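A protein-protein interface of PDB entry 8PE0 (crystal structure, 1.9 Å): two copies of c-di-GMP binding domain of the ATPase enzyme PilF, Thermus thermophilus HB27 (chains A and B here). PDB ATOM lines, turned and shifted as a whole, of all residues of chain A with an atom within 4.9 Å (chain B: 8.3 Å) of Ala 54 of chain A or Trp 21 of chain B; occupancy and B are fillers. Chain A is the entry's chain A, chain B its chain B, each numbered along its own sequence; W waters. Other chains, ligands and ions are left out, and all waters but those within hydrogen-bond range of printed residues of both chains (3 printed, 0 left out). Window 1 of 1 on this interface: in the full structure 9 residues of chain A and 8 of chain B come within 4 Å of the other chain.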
ATOM      1  N   LEU A  16     -16.101 -14.968  16.054  1.00  0.00           N
ATOM      2  CA  LEU A  16     -16.300 -14.260  17.320  1.00  0.00           C
ATOM      3  C   LEU A  16     -15.291 -13.139  17.481  1.00  0.00           C
ATOM      4  O   LEU A  16     -15.618 -12.080  18.034  1.00  0.00           O
ATOM      5  CB  LEU A  16     -16.213 -15.231  18.498  1.00  0.00           C
ATOM      6  CG  LEU A  16     -17.384 -16.230  18.580  1.00  0.00           C
ATOM      7  CD1 LEU A  16     -17.002 -17.376  19.497  1.00  0.00           C
ATOM      8  CD2 LEU A  16     -18.720 -15.550  19.046  1.00  0.00           C
ATOM      9  N   GLY A  20     -15.962  -8.981  17.696  1.00  0.00           N
ATOM     10  CA  GLY A  20     -15.602  -8.338  18.947  1.00  0.00           C
ATOM     11  C   GLY A  20     -16.242  -8.925  20.185  1.00  0.00           C
ATOM     12  O   GLY A  20     -16.305  -8.247  21.212  1.00  0.00           O
ATOM     13  N   TRP A  21     -16.729 -10.165  20.126  1.00  0.00           N
ATOM     14  CA  TRP A  21     -17.403 -10.783  21.259  1.00  0.00           C
ATOM     15  C   TRP A  21     -16.495 -11.703  22.058  1.00  0.00           C
ATOM     16  O   TRP A  21     -16.903 -12.177  23.122  1.00  0.00           O
ATOM     17  CB  TRP A  21     -18.637 -11.571  20.785  1.00  0.00           C
ATOM     18  CG  TRP A  21     -19.675 -10.705  20.190  1.00  0.00           C
ATOM     19  CD1 TRP A  21     -19.838  -9.361  20.384  1.00  0.00           C
ATOM     20  CD2 TRP A  21     -20.705 -11.111  19.289  1.00  0.00           C
ATOM     21  NE1 TRP A  21     -20.908  -8.908  19.646  1.00  0.00           N
ATOM     22  CE2 TRP A  21     -21.454  -9.964  18.968  1.00  0.00           C
ATOM     23  CE3 TRP A  21     -21.054 -12.334  18.711  1.00  0.00           C
ATOM     24  CZ2 TRP A  21     -22.545 -10.004  18.103  1.00  0.00           C
ATOM     25  CZ3 TRP A  21     -22.134 -12.373  17.853  1.00  0.00           C
ATOM     26  CH2 TRP A  21     -22.872 -11.212  17.564  1.00  0.00           C
ATOM     27  N   LEU A  50     -18.628 -16.392  27.570  1.00  0.00           N
ATOM     28  CA  LEU A  50     -19.237 -15.925  26.331  1.00  0.00           C
ATOM     29  C   LEU A  50     -20.750 -16.040  26.448  1.00  0.00           C
ATOM     30  O   LEU A  50     -21.242 -17.097  26.863  1.00  0.00           O
ATOM     31  CB  LEU A  50     -18.735 -16.766  25.162  1.00  0.00           C
ATOM     32  CG  LEU A  50     -19.387 -16.423  23.828  1.00  0.00           C
ATOM     33  CD1 LEU A  50     -18.890 -15.077  23.330  1.00  0.00           C
ATOM     34  CD2 LEU A  50     -19.095 -17.514  22.810  1.00  0.00           C
ATOM     35  N   PRO A  51     -21.524 -14.985  26.139  1.00  0.00           N
ATOM     36  CA  PRO A  51     -22.985 -15.125  26.182  1.00  0.00           C
ATOM     37  C   PRO A  51     -23.444 -16.170  25.195  1.00  0.00           C
ATOM     38  O   PRO A  51     -22.985 -16.210  24.049  1.00  0.00           O
ATOM     39  CB  PRO A  51     -23.503 -13.733  25.797  1.00  0.00           C
ATOM     40  CG  PRO A  51     -22.392 -12.786  26.238  1.00  0.00           C
ATOM     41  CD  PRO A  51     -21.112 -13.578  25.960  1.00  0.00           C
ATOM     42  N   GLU A  52     -24.387 -17.005  25.638  1.00  0.00           N
ATOM     43  CA  GLU A  52     -24.893 -18.061  24.759  1.00  0.00           C
ATOM     44  C   GLU A  52     -25.493 -17.484  23.478  1.00  0.00           C
ATOM     45  O   GLU A  52     -25.372 -18.072  22.402  1.00  0.00           O
ATOM     46  CB  GLU A  52     -25.932 -18.900  25.507  1.00  0.00           C
ATOM     47  CG  GLU A  52     -26.409 -20.121  24.738  1.00  0.00           C
ATOM     48  CD  GLU A  52     -27.048 -21.161  25.639  1.00  0.00           C
ATOM     49  OE2 GLU A  52     -26.297 -21.894  26.317  1.00  0.00           O
ATOM     50  N   GLU A  53     -26.145 -16.330  23.568  1.00  0.00           N
ATOM     51  CA  GLU A  53     -26.679 -15.745  22.343  1.00  0.00           C
ATOM     52  C   GLU A  53     -25.572 -15.291  21.394  1.00  0.00           C
ATOM     53  O   GLU A  53     -25.764 -15.289  20.173  1.00  0.00           O
ATOM     54  CB  GLU A  53     -27.601 -14.578  22.685  1.00  0.00           C
ATOM     55  CG  GLU A  53     -28.546 -14.268  21.581  1.00  0.00           C
ATOM     56  CD  GLU A  53     -29.406 -13.087  21.882  1.00  0.00           C
ATOM     57  OE1 GLU A  53     -28.989 -11.956  21.552  1.00  0.00           O
ATOM     58  OE2 GLU A  53     -30.500 -13.298  22.453  1.00  0.00           O
ATOM     59  N   ALA A  54     -24.414 -14.902  21.922  1.00  0.00           N
ATOM     60  CA  ALA A  54     -23.289 -14.572  21.042  1.00  0.00           C
ATOM     61  C   ALA A  54     -22.803 -15.810  20.297  1.00  0.00           C
ATOM     62  O   ALA A  54     -22.529 -15.767  19.083  1.00  0.00           O
ATOM     63  CB  ALA A  54     -22.153 -13.934  21.861  1.00  0.00           C
ATOM     64  N   LEU A  55     -22.700 -16.930  21.001  1.00  0.00           N
ATOM     65  CA  LEU A  55     -22.355 -18.184  20.346  1.00  0.00           C
ATOM     66  C   LEU A  55     -23.339 -18.500  19.222  1.00  0.00           C
ATOM     67  O   LEU A  55     -22.939 -18.812  18.098  1.00  0.00           O
ATOM     68  CB  LEU A  55     -22.328 -19.315  21.377  1.00  0.00           C
ATOM     69  CG  LEU A  55     -22.077 -20.716  20.790  1.00  0.00           C
ATOM     70  CD1 LEU A  55     -20.733 -20.732  20.098  1.00  0.00           C
ATOM     71  CD2 LEU A  55     -22.126 -21.792  21.875  1.00  0.00           C
ATOM     72  N   TYR A  56     -24.640 -18.417  19.500  1.00  0.00           N
ATOM     73  CA  TYR A  56     -25.606 -18.841  18.483  1.00  0.00           C
ATOM     74  C   TYR A  56     -25.657 -17.872  17.310  1.00  0.00           C
ATOM     75  O   TYR A  56     -25.826 -18.297  16.163  1.00  0.00           O
ATOM     76  CB  TYR A  56     -26.997 -19.006  19.100  1.00  0.00           C
ATOM     77  CG  TYR A  56     -27.199 -20.404  19.630  1.00  0.00           C
ATOM     78  CD1 TYR A  56     -26.394 -20.894  20.652  1.00  0.00           C
ATOM     79  CD2 TYR A  56     -28.195 -21.238  19.115  1.00  0.00           C
ATOM     80  CE1 TYR A  56     -26.566 -22.175  21.150  1.00  0.00           C
ATOM     81  CE2 TYR A  56     -28.383 -22.520  19.611  1.00  0.00           C
ATOM     82  CZ  TYR A  56     -27.561 -22.986  20.624  1.00  0.00           C
ATOM     83  OH  TYR A  56     -27.723 -24.259  21.122  1.00  0.00           O
ATOM     84  N   ARG A  57     -25.532 -16.571  17.567  1.00  0.00           N
ATOM     85  CA  ARG A  57     -25.474 -15.624  16.452  1.00  0.00           C
ATOM     86  C   ARG A  57     -24.280 -15.911  15.535  1.00  0.00           C
ATOM     87  O   ARG A  57     -24.410 -15.856  14.305  1.00  0.00           O
ATOM     88  CB  ARG A  57     -25.405 -14.192  16.973  1.00  0.00           C
ATOM     89  CG  ARG A  57     -26.754 -13.638  17.460  1.00  0.00           C
ATOM     90  CD  ARG A  57     -26.560 -12.259  18.087  1.00  0.00           C
ATOM     91  NE  ARG A  57     -27.781 -11.820  18.766  1.00  0.00           N
ATOM     92  CZ  ARG A  57     -28.821 -11.272  18.149  1.00  0.00           C
ATOM     93  NH1 ARG A  57     -28.785 -11.089  16.836  1.00  0.00           N
ATOM     94  NH2 ARG A  57     -29.890 -10.893  18.845  1.00  0.00           N
ATOM     95  N   ALA A  58     -23.113 -16.221  16.112  1.00  0.00           N
ATOM     96  CA  ALA A  58     -21.948 -16.567  15.294  1.00  0.00           C
ATOM     97  C   ALA A  58     -22.165 -17.859  14.518  1.00  0.00           C
ATOM     98  O   ALA A  58     -21.792 -17.952  13.343  1.00  0.00           O
ATOM     99  CB  ALA A  58     -20.704 -16.717  16.164  1.00  0.00           C
ATOM    100  N   GLY B  13     -22.242   0.281  30.800  1.00  0.00           N
ATOM    101  CA  GLY B  13     -20.976  -0.298  30.364  1.00  0.00           C
ATOM    102  C   GLY B  13     -20.533  -1.436  31.260  1.00  0.00           C
ATOM    103  O   GLY B  13     -20.068  -2.474  30.778  1.00  0.00           O
ATOM    104  N   GLU B  14     -20.743  -1.284  32.567  1.00  0.00           N
ATOM    105  CA  GLU B  14     -20.396  -2.340  33.512  1.00  0.00           C
ATOM    106  C   GLU B  14     -21.276  -3.571  33.325  1.00  0.00           C
ATOM    107  O   GLU B  14     -20.787  -4.700  33.416  1.00  0.00           O
ATOM    108  CB  GLU B  14     -20.510  -1.823  34.952  1.00  0.00           C
ATOM    109  CG  GLU B  14     -19.502  -0.739  35.305  1.00  0.00           C
ATOM    110  CD  GLU B  14     -19.722  -0.151  36.699  1.00  0.00           C
ATOM    111  OE1 GLU B  14     -20.898  -0.024  37.132  1.00  0.00           O
ATOM    112  OE2 GLU B  14     -18.710   0.186  37.356  1.00  0.00           O
ATOM    113  N   LEU B  15     -22.580  -3.376  33.086  1.00  0.00           N
ATOM    114  CA  LEU B  15     -23.458  -4.523  32.869  1.00  0.00           C
ATOM    115  C   LEU B  15     -23.026  -5.324  31.647  1.00  0.00           C
ATOM    116  O   LEU B  15     -22.955  -6.553  31.697  1.00  0.00           O
ATOM    117  CB  LEU B  15     -24.914  -4.065  32.720  1.00  0.00           C
ATOM    118  CG  LEU B  15     -25.687  -3.832  34.023  1.00  0.00           C
ATOM    119  CD1 LEU B  15     -26.778  -2.777  33.826  1.00  0.00           C
ATOM    120  CD2 LEU B  15     -26.280  -5.144  34.525  1.00  0.00           C
ATOM    121  N   LEU B  16     -22.707  -4.640  30.549  1.00  0.00           N
ATOM    122  CA  LEU B  16     -22.293  -5.340  29.340  1.00  0.00           C
ATOM    123  C   LEU B  16     -20.926  -5.988  29.499  1.00  0.00           C
ATOM    124  O   LEU B  16     -20.669  -7.049  28.917  1.00  0.00           O
ATOM    125  CB  LEU B  16     -22.301  -4.370  28.163  1.00  0.00           C
ATOM    126  CG  LEU B  16     -23.723  -3.909  27.866  1.00  0.00           C
ATOM    127  CD1 LEU B  16     -23.677  -2.715  26.947  1.00  0.00           C
ATOM    128  CD2 LEU B  16     -24.561  -5.075  27.253  1.00  0.00           C
ATOM    129  N   LEU B  17     -20.043  -5.369  30.275  1.00  0.00           N
ATOM    130  CA  LEU B  17     -18.734  -5.957  30.537  1.00  0.00           C
ATOM    131  C   LEU B  17     -18.873  -7.255  31.317  1.00  0.00           C
ATOM    132  O   LEU B  17     -18.249  -8.272  30.988  1.00  0.00           O
ATOM    133  CB  LEU B  17     -17.878  -4.958  31.319  1.00  0.00           C
ATOM    134  CG  LEU B  17     -16.708  -4.311  30.592  1.00  0.00           C
ATOM    135  CD1 LEU B  17     -15.995  -3.333  31.528  1.00  0.00           C
ATOM    136  CD2 LEU B  17     -15.757  -5.372  30.108  1.00  0.00           C
ATOM    137  N   GLN B  18     -19.695  -7.228  32.364  1.00  0.00           N
ATOM    138  CA  GLN B  18     -19.923  -8.406  33.190  1.00  0.00           C
ATOM    139  C   GLN B  18     -20.500  -9.554  32.364  1.00  0.00           C
ATOM    140  O   GLN B  18     -20.135 -10.716  32.566  1.00  0.00           O
ATOM    141  CB  GLN B  18     -20.846  -8.011  34.342  1.00  0.00           C
ATOM    142  CG  GLN B  18     -21.310  -9.105  35.274  1.00  0.00           C
ATOM    143  CD  GLN B  18     -22.373  -8.588  36.251  1.00  0.00           C
ATOM    144  OE1 GLN B  18     -22.182  -8.613  37.467  1.00  0.00           O
ATOM    145  NE2 GLN B  18     -23.488  -8.102  35.714  1.00  0.00           N
ATOM    146  N   LYS B  19     -21.391  -9.241  31.421  1.00  0.00           N
ATOM    147  CA  LYS B  19     -21.968 -10.278  30.572  1.00  0.00           C
ATOM    148  C   LYS B  19     -20.964 -10.800  29.552  1.00  0.00           C
ATOM    149  O   LYS B  19     -21.031 -11.969  29.156  1.00  0.00           O
ATOM    150  CB  LYS B  19     -23.209  -9.729  29.870  1.00  0.00           C
ATOM    151  CG  LYS B  19     -24.444  -9.744  30.744  1.00  0.00           C
ATOM    152  CD  LYS B  19     -25.430  -8.653  30.348  1.00  0.00           C
ATOM    153  N   GLY B  20     -20.025  -9.964  29.125  1.00  0.00           N
ATOM    154  CA  GLY B  20     -19.040 -10.363  28.147  1.00  0.00           C
ATOM    155  C   GLY B  20     -19.330  -9.911  26.737  1.00  0.00           C
ATOM    156  O   GLY B  20     -18.665 -10.374  25.809  1.00  0.00           O
ATOM    157  N   TRP B  21     -20.299  -9.016  26.545  1.00  0.00           N
ATOM    158  CA  TRP B  21     -20.635  -8.561  25.201  1.00  0.00           C
ATOM    159  C   TRP B  21     -19.610  -7.595  24.625  1.00  0.00           C
ATOM    160  O   TRP B  21     -19.542  -7.445  23.398  1.00  0.00           O
ATOM    161  CB  TRP B  21     -22.002  -7.893  25.216  1.00  0.00           C
ATOM    162  CG  TRP B  21     -23.147  -8.846  25.134  1.00  0.00           C
ATOM    163  CD1 TRP B  21     -24.056  -9.121  26.119  1.00  0.00           C
ATOM    164  CD2 TRP B  21     -23.534  -9.630  23.993  1.00  0.00           C
ATOM    165  NE1 TRP B  21     -24.969 -10.042  25.666  1.00  0.00           N
ATOM    166  CE2 TRP B  21     -24.678 -10.362  24.363  1.00  0.00           C
ATOM    167  CE3 TRP B  21     -23.018  -9.785  22.699  1.00  0.00           C
ATOM    168  CZ2 TRP B  21     -25.331 -11.233  23.481  1.00  0.00           C
ATOM    169  CZ3 TRP B  21     -23.670 -10.653  21.823  1.00  0.00           C
ATOM    170  CH2 TRP B  21     -24.807 -11.368  22.224  1.00  0.00           C
ATOM    171  N   ILE B  22     -18.828  -6.925  25.477  1.00  0.00           N
ATOM    172  CA  ILE B  22     -17.833  -5.949  25.053  1.00  0.00           C
ATOM    173  C   ILE B  22     -16.575  -6.154  25.885  1.00  0.00           C
ATOM    174  O   ILE B  22     -16.621  -6.673  27.004  1.00  0.00           O
ATOM    175  CB  ILE B  22     -18.328  -4.491  25.227  1.00  0.00           C
ATOM    176  CG1 ILE B  22     -18.546  -4.172  26.713  1.00  0.00           C
ATOM    177  CG2 ILE B  22     -19.608  -4.238  24.437  1.00  0.00           C
ATOM    178  CD1 ILE B  22     -18.977  -2.720  26.977  1.00  0.00           C
ATOM    179  N   SER B  23     -15.448  -5.698  25.347  1.00  0.00           N
ATOM    180  CA  SER B  23     -14.204  -5.690  26.101  1.00  0.00           C
ATOM    181  C   SER B  23     -14.030  -4.362  26.833  1.00  0.00           C
ATOM    182  O   SER B  23     -14.712  -3.371  26.554  1.00  0.00           O
ATOM    183  CB  SER B  23     -13.010  -5.939  25.178  1.00  0.00           C
ATOM    184  OG  SER B  23     -12.913  -4.891  24.231  1.00  0.00           O
ATOM    185  N   ARG B  24     -13.101  -4.350  27.791  1.00  0.00           N
ATOM    186  CA  ARG B  24     -12.817  -3.106  28.496  1.00  0.00           C
ATOM    187  C   ARG B  24     -12.281  -2.047  27.539  1.00  0.00           C
ATOM    188  O   ARG B  24     -12.644  -0.871  27.641  1.00  0.00           O
ATOM    189  CB  ARG B  24     -11.845  -3.356  29.651  1.00  0.00           C
ATOM    190  CG  ARG B  24     -12.055  -4.687  30.357  1.00  0.00           C
ATOM    191  CD  ARG B  24     -11.365  -4.733  31.718  1.00  0.00           C
ATOM    192  NE  ARG B  24     -12.255  -4.269  32.783  1.00  0.00           N
ATOM    193  CZ  ARG B  24     -11.979  -3.264  33.610  1.00  0.00           C
ATOM    194  NH1 ARG B  24     -12.853  -2.910  34.543  1.00  0.00           N
ATOM    195  NH2 ARG B  24     -10.823  -2.621  33.510  1.00  0.00           N
ATOM    196  N   ALA B  26     -12.946  -1.802  24.279  1.00  0.00           N
ATOM    197  CA  ALA B  26     -14.070  -1.314  23.484  1.00  0.00           C
ATOM    198  C   ALA B  26     -14.924  -0.326  24.274  1.00  0.00           C
ATOM    199  O   ALA B  26     -15.431   0.654  23.712  1.00  0.00           O
ATOM    200  CB  ALA B  26     -14.925  -2.485  23.001  1.00  0.00           C
ATOM    201  N   LEU B  45     -22.137   1.462  21.042  1.00  0.00           N
ATOM    202  CA  LEU B  45     -21.819   0.042  21.135  1.00  0.00           C
ATOM    203  C   LEU B  45     -22.566  -0.757  20.081  1.00  0.00           C
ATOM    204  O   LEU B  45     -22.011  -1.703  19.509  1.00  0.00           O
ATOM    205  CB  LEU B  45     -22.136  -0.481  22.539  1.00  0.00           C
ATOM    206  CG  LEU B  45     -21.237   0.168  23.603  1.00  0.00           C
ATOM    207  CD1 LEU B  45     -21.668  -0.237  25.017  1.00  0.00           C
ATOM    208  CD2 LEU B  45     -19.767  -0.197  23.363  1.00  0.00           C
ATOM    209  N   LYS B  48     -20.899  -0.513  16.915  1.00  0.00           N
ATOM    210  CA  LYS B  48     -19.651  -1.273  16.949  1.00  0.00           C
ATOM    211  C   LYS B  48     -19.853  -2.789  17.064  1.00  0.00           C
ATOM    212  O   LYS B  48     -18.870  -3.518  17.248  1.00  0.00           O
ATOM    213  CB  LYS B  48     -18.783  -0.786  18.111  1.00  0.00           C
ATOM    214  CG  LYS B  48     -18.251   0.635  17.952  1.00  0.00           C
ATOM    215  CD  LYS B  48     -17.386   1.029  19.142  1.00  0.00           C
ATOM    216  CE  LYS B  48     -16.432   2.160  18.789  1.00  0.00           C
ATOM    217  NZ  LYS B  48     -16.077   2.145  17.342  1.00  0.00           N
ATOM    218  N   GLY B  49     -21.088  -3.285  16.981  1.00  0.00           N
ATOM    219  CA  GLY B  49     -21.321  -4.727  16.900  1.00  0.00           C
ATOM    220  C   GLY B  49     -22.183  -5.319  18.004  1.00  0.00           C
ATOM    221  O   GLY B  49     -22.467  -6.523  17.963  1.00  0.00           O
ATOM    222  N   LEU B  50     -22.598  -4.569  18.997  1.00  0.00           N
ATOM    223  CA  LEU B  50     -23.490  -5.120  20.023  1.00  0.00           C
ATOM    224  C   LEU B  50     -24.897  -5.309  19.459  1.00  0.00           C
ATOM    225  O   LEU B  50     -25.458  -4.367  18.892  1.00  0.00           O
ATOM    226  CB  LEU B  50     -23.539  -4.183  21.218  1.00  0.00           C
ATOM    227  CG  LEU B  50     -24.472  -4.531  22.382  1.00  0.00           C
ATOM    228  CD1 LEU B  50     -23.976  -5.773  23.081  1.00  0.00           C
ATOM    229  CD2 LEU B  50     -24.542  -3.343  23.367  1.00  0.00           C
ATOM    230  N   PRO B  51     -25.495  -6.493  19.584  1.00  0.00           N
ATOM    231  CA  PRO B  51     -26.877  -6.657  19.110  1.00  0.00           C
ATOM    232  C   PRO B  51     -27.821  -5.741  19.876  1.00  0.00           C
ATOM    233  O   PRO B  51     -27.724  -5.594  21.097  1.00  0.00           O
ATOM    234  CB  PRO B  51     -27.185  -8.139  19.375  1.00  0.00           C
ATOM    235  CG  PRO B  51     -25.853  -8.823  19.386  1.00  0.00           C
ATOM    236  CD  PRO B  51     -24.867  -7.774  19.949  1.00  0.00           C
ATOM    237  N   GLU B  52     -28.744  -5.113  19.145  1.00  0.00           N
ATOM    238  CA  GLU B  52     -29.673  -4.208  19.816  1.00  0.00           C
ATOM    239  C   GLU B  52     -30.488  -4.946  20.869  1.00  0.00           C
ATOM    240  O   GLU B  52     -30.826  -4.369  21.906  1.00  0.00           O
ATOM    241  CB  GLU B  52     -30.585  -3.523  18.794  1.00  0.00           C
ATOM    242  CG  GLU B  52     -31.367  -2.351  19.371  1.00  0.00           C
ATOM    243  CD  GLU B  52     -31.516  -1.188  18.402  1.00  0.00           C
ATOM    244  OE2 GLU B  52     -31.954  -0.099  18.844  1.00  0.00           O
ATOM    245  N   GLU B  53     -30.789  -6.231  20.637  1.00  0.00           N
ATOM    246  CA  GLU B  53     -31.508  -6.990  21.657  1.00  0.00           C
ATOM    247  C   GLU B  53     -30.681  -7.152  22.931  1.00  0.00           C
ATOM    248  O   GLU B  53     -31.230  -7.131  24.036  1.00  0.00           O
ATOM    249  CB  GLU B  53     -31.917  -8.358  21.112  1.00  0.00           C
ATOM    250  CG  GLU B  53     -32.866  -8.309  19.920  1.00  0.00           C
ATOM    251  CD  GLU B  53     -32.174  -8.104  18.567  1.00  0.00           C
ATOM    252  OE1 GLU B  53     -32.892  -8.170  17.542  1.00  0.00           O
ATOM    253  OE2 GLU B  53     -30.939  -7.873  18.518  1.00  0.00           O
ATOM    254  N   ALA B  54     -29.359  -7.337  22.806  1.00  0.00           N
ATOM    255  CA  ALA B  54     -28.529  -7.403  24.008  1.00  0.00           C
ATOM    256  C   ALA B  54     -28.506  -6.064  24.731  1.00  0.00           C
ATOM    257  O   ALA B  54     -28.479  -6.009  25.970  1.00  0.00           O
ATOM    258  CB  ALA B  54     -27.107  -7.849  23.655  1.00  0.00           C
ATOM    259  N   LEU B  55     -28.506  -4.967  23.975  1.00  0.00           N
ATOM    260  CA  LEU B  55     -28.497  -3.661  24.611  1.00  0.00           C
ATOM    261  C   LEU B  55     -29.755  -3.472  25.441  1.00  0.00           C
ATOM    262  O   LEU B  55     -29.695  -3.023  26.591  1.00  0.00           O
ATOM    263  CB  LEU B  55     -28.387  -2.562  23.556  1.00  0.00           C
ATOM    264  CG  LEU B  55     -28.664  -1.164  24.110  1.00  0.00           C
ATOM    265  CD1 LEU B  55     -27.666  -0.802  25.203  1.00  0.00           C
ATOM    266  CD2 LEU B  55     -28.633  -0.114  22.992  1.00  0.00           C
ATOM    267  N   ARG B  57     -31.849  -5.765  26.694  1.00  0.00           N
ATOM    268  CA  ARG B  57     -31.943  -6.638  27.862  1.00  0.00           C
ATOM    269  C   ARG B  57     -31.147  -6.068  29.033  1.00  0.00           C
ATOM    270  O   ARG B  57     -31.608  -6.108  30.183  1.00  0.00           O
ATOM    271  CB  ARG B  57     -31.475  -8.063  27.518  1.00  0.00           C
ATOM    272  CG  ARG B  57     -32.467  -8.903  26.705  1.00  0.00           C
ATOM    273  CD  ARG B  57     -32.123 -10.408  26.754  1.00  0.00           C
ATOM    274  NE  ARG B  57     -30.825 -10.637  26.146  1.00  0.00           N
ATOM    275  CZ  ARG B  57     -30.629 -10.778  24.837  1.00  0.00           C
ATOM    276  NH1 ARG B  57     -31.662 -10.744  23.999  1.00  0.00           N
ATOM    277  NH2 ARG B  57     -29.400 -10.965  24.367  1.00  0.00           N
ATOM    278  N   ALA B  58     -29.958  -5.502  28.756  1.00  0.00           N
ATOM    279  CA  ALA B  58     -29.165  -4.861  29.805  1.00  0.00           C
ATOM    280  C   ALA B  58     -29.872  -3.633  30.375  1.00  0.00           C
ATOM    281  O   ALA B  58     -29.873  -3.418  31.594  1.00  0.00           O
ATOM    282  CB  ALA B  58     -27.793  -4.463  29.255  1.00  0.00           C
HETATM  283  O   HOH W   1     -17.238 -12.681  25.994  1.00  0.00           O
HETATM  284  O   HOH W   2     -15.981  -5.488  21.910  1.00  0.00           O
HETATM  285  O   HOH W   3     -20.404  -6.052  21.107  1.00  0.00           O
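Water W1 lies within hydrogen-bond range of O of Gly 20 of chain B (2.7 Å) and O of Trp 21 of chain A (2.9 Å). Water W3 lies within hydrogen-bond range of O of Trp 21 of chain B (2.8 Å), NE1 of Trp 21 of chain A (3.2 Å) and N of Leu 50 of chain B (3.4 Å). Water W2 lies within hydrogen-bond range of O of Gly 20 of chain A and N of Ser 23 of chain B.
Trp 21 of chain A touches its own counterpart, Trp 21 of chain B. Trp 21 of chain A touches Pro 51 of chain B, and with the chains exchanged Pro 51 of chain A touches Trp 21 of chain B. Glu 53 of chain A touches Arg 57 of chain B, and with the chains exchanged Arg 57 of chain A touches Glu 53 of chain B. Ala 54 of chain A touches Trp 21 of chain B, but with the chains exchanged Trp 21 of chain A does not touch Ala 54 of chain B (7.5 Å). Positions printed for both chains: 16, 20, 21, 50, 51, 52, 53, 54, 55, 57 and 58.
Ala 54 of chain A touches one residue of chain B. Of the printed residues of chain A, Gly 20 of chain B touches Trp 21 (3.7 Å). Of the printed residues of chain A, Trp 21 of chain B touches Gly 20, Trp 21, Pro 51 and Ala 54. Of the printed residues of chain A, Pro 51 of chain B touches Trp 21 and Arg 57. Glu 52 of chain B touches none of the printed residues of chain A.
Printed residues of chain A that touch a printed residue of chain B: Gly 20, Trp 21, Pro 51, Glu 53, Ala 54 and Arg 57. Hydrophobic or aromatic side chains of chain A within 4 Å of the printed part of chain B: Trp 21, Pro 51 and Ala 54. Among the printed residues, 11 pairs touch across the chains.
Among the printed residues, merely in contact across the chains: Gly 20 of chain A with Trp 21 of chain B (3.99 Å), Trp 21 of chain A with Gly 20 of chain B (3.7 Å), Trp 21 of chain A with Trp 21 of chain B (3.6 Å), Trp 21 of chain A with Pro 51 of chain B (3.7 Å), Pro 51 of chain A with Lys 19 of chain B (3.3 Å), Pro 51 of chain A with Trp 21 of chain B (3.8 Å), Ala 54 of chain A with Trp 21 of chain B (3.6 Å) and Arg 57 of chain A with Pro 51 of chain B (3.6 Å).
The backbone carbonyl oxygen (O) of Leu 16 of chain B is in hydrogen-bond range of the backbone NH (N) of Trp 21 of chain B. OE1 of Glu 53 of chain A is in salt-bridge range of NE of Arg 57 of chain A (3.0 Å). The backbone carbonyl oxygen of Leu 16 of chain A sits at hydrogen-bond distance from the backbone NH of Trp 21 of chain A (3.0 Å).
The side-chain carboxylate (OE1) of Glu 53 of chain A lies within salt-bridge range of the guanidinium group (NH2) of Arg 57 of chain B (3.0 Å). The guanidinium group (NH2) of Arg 57 of chain A is in salt-bridge range of the side-chain carboxylate (OE2) of Glu 53 of chain B, 3.2 Å away. The indole nitrogen (NE1) of Trp 21 of chain A lies within hydrogen-bond range of the backbone carbonyl oxygen (O) of Gly 49 of chain B (3.3 Å).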
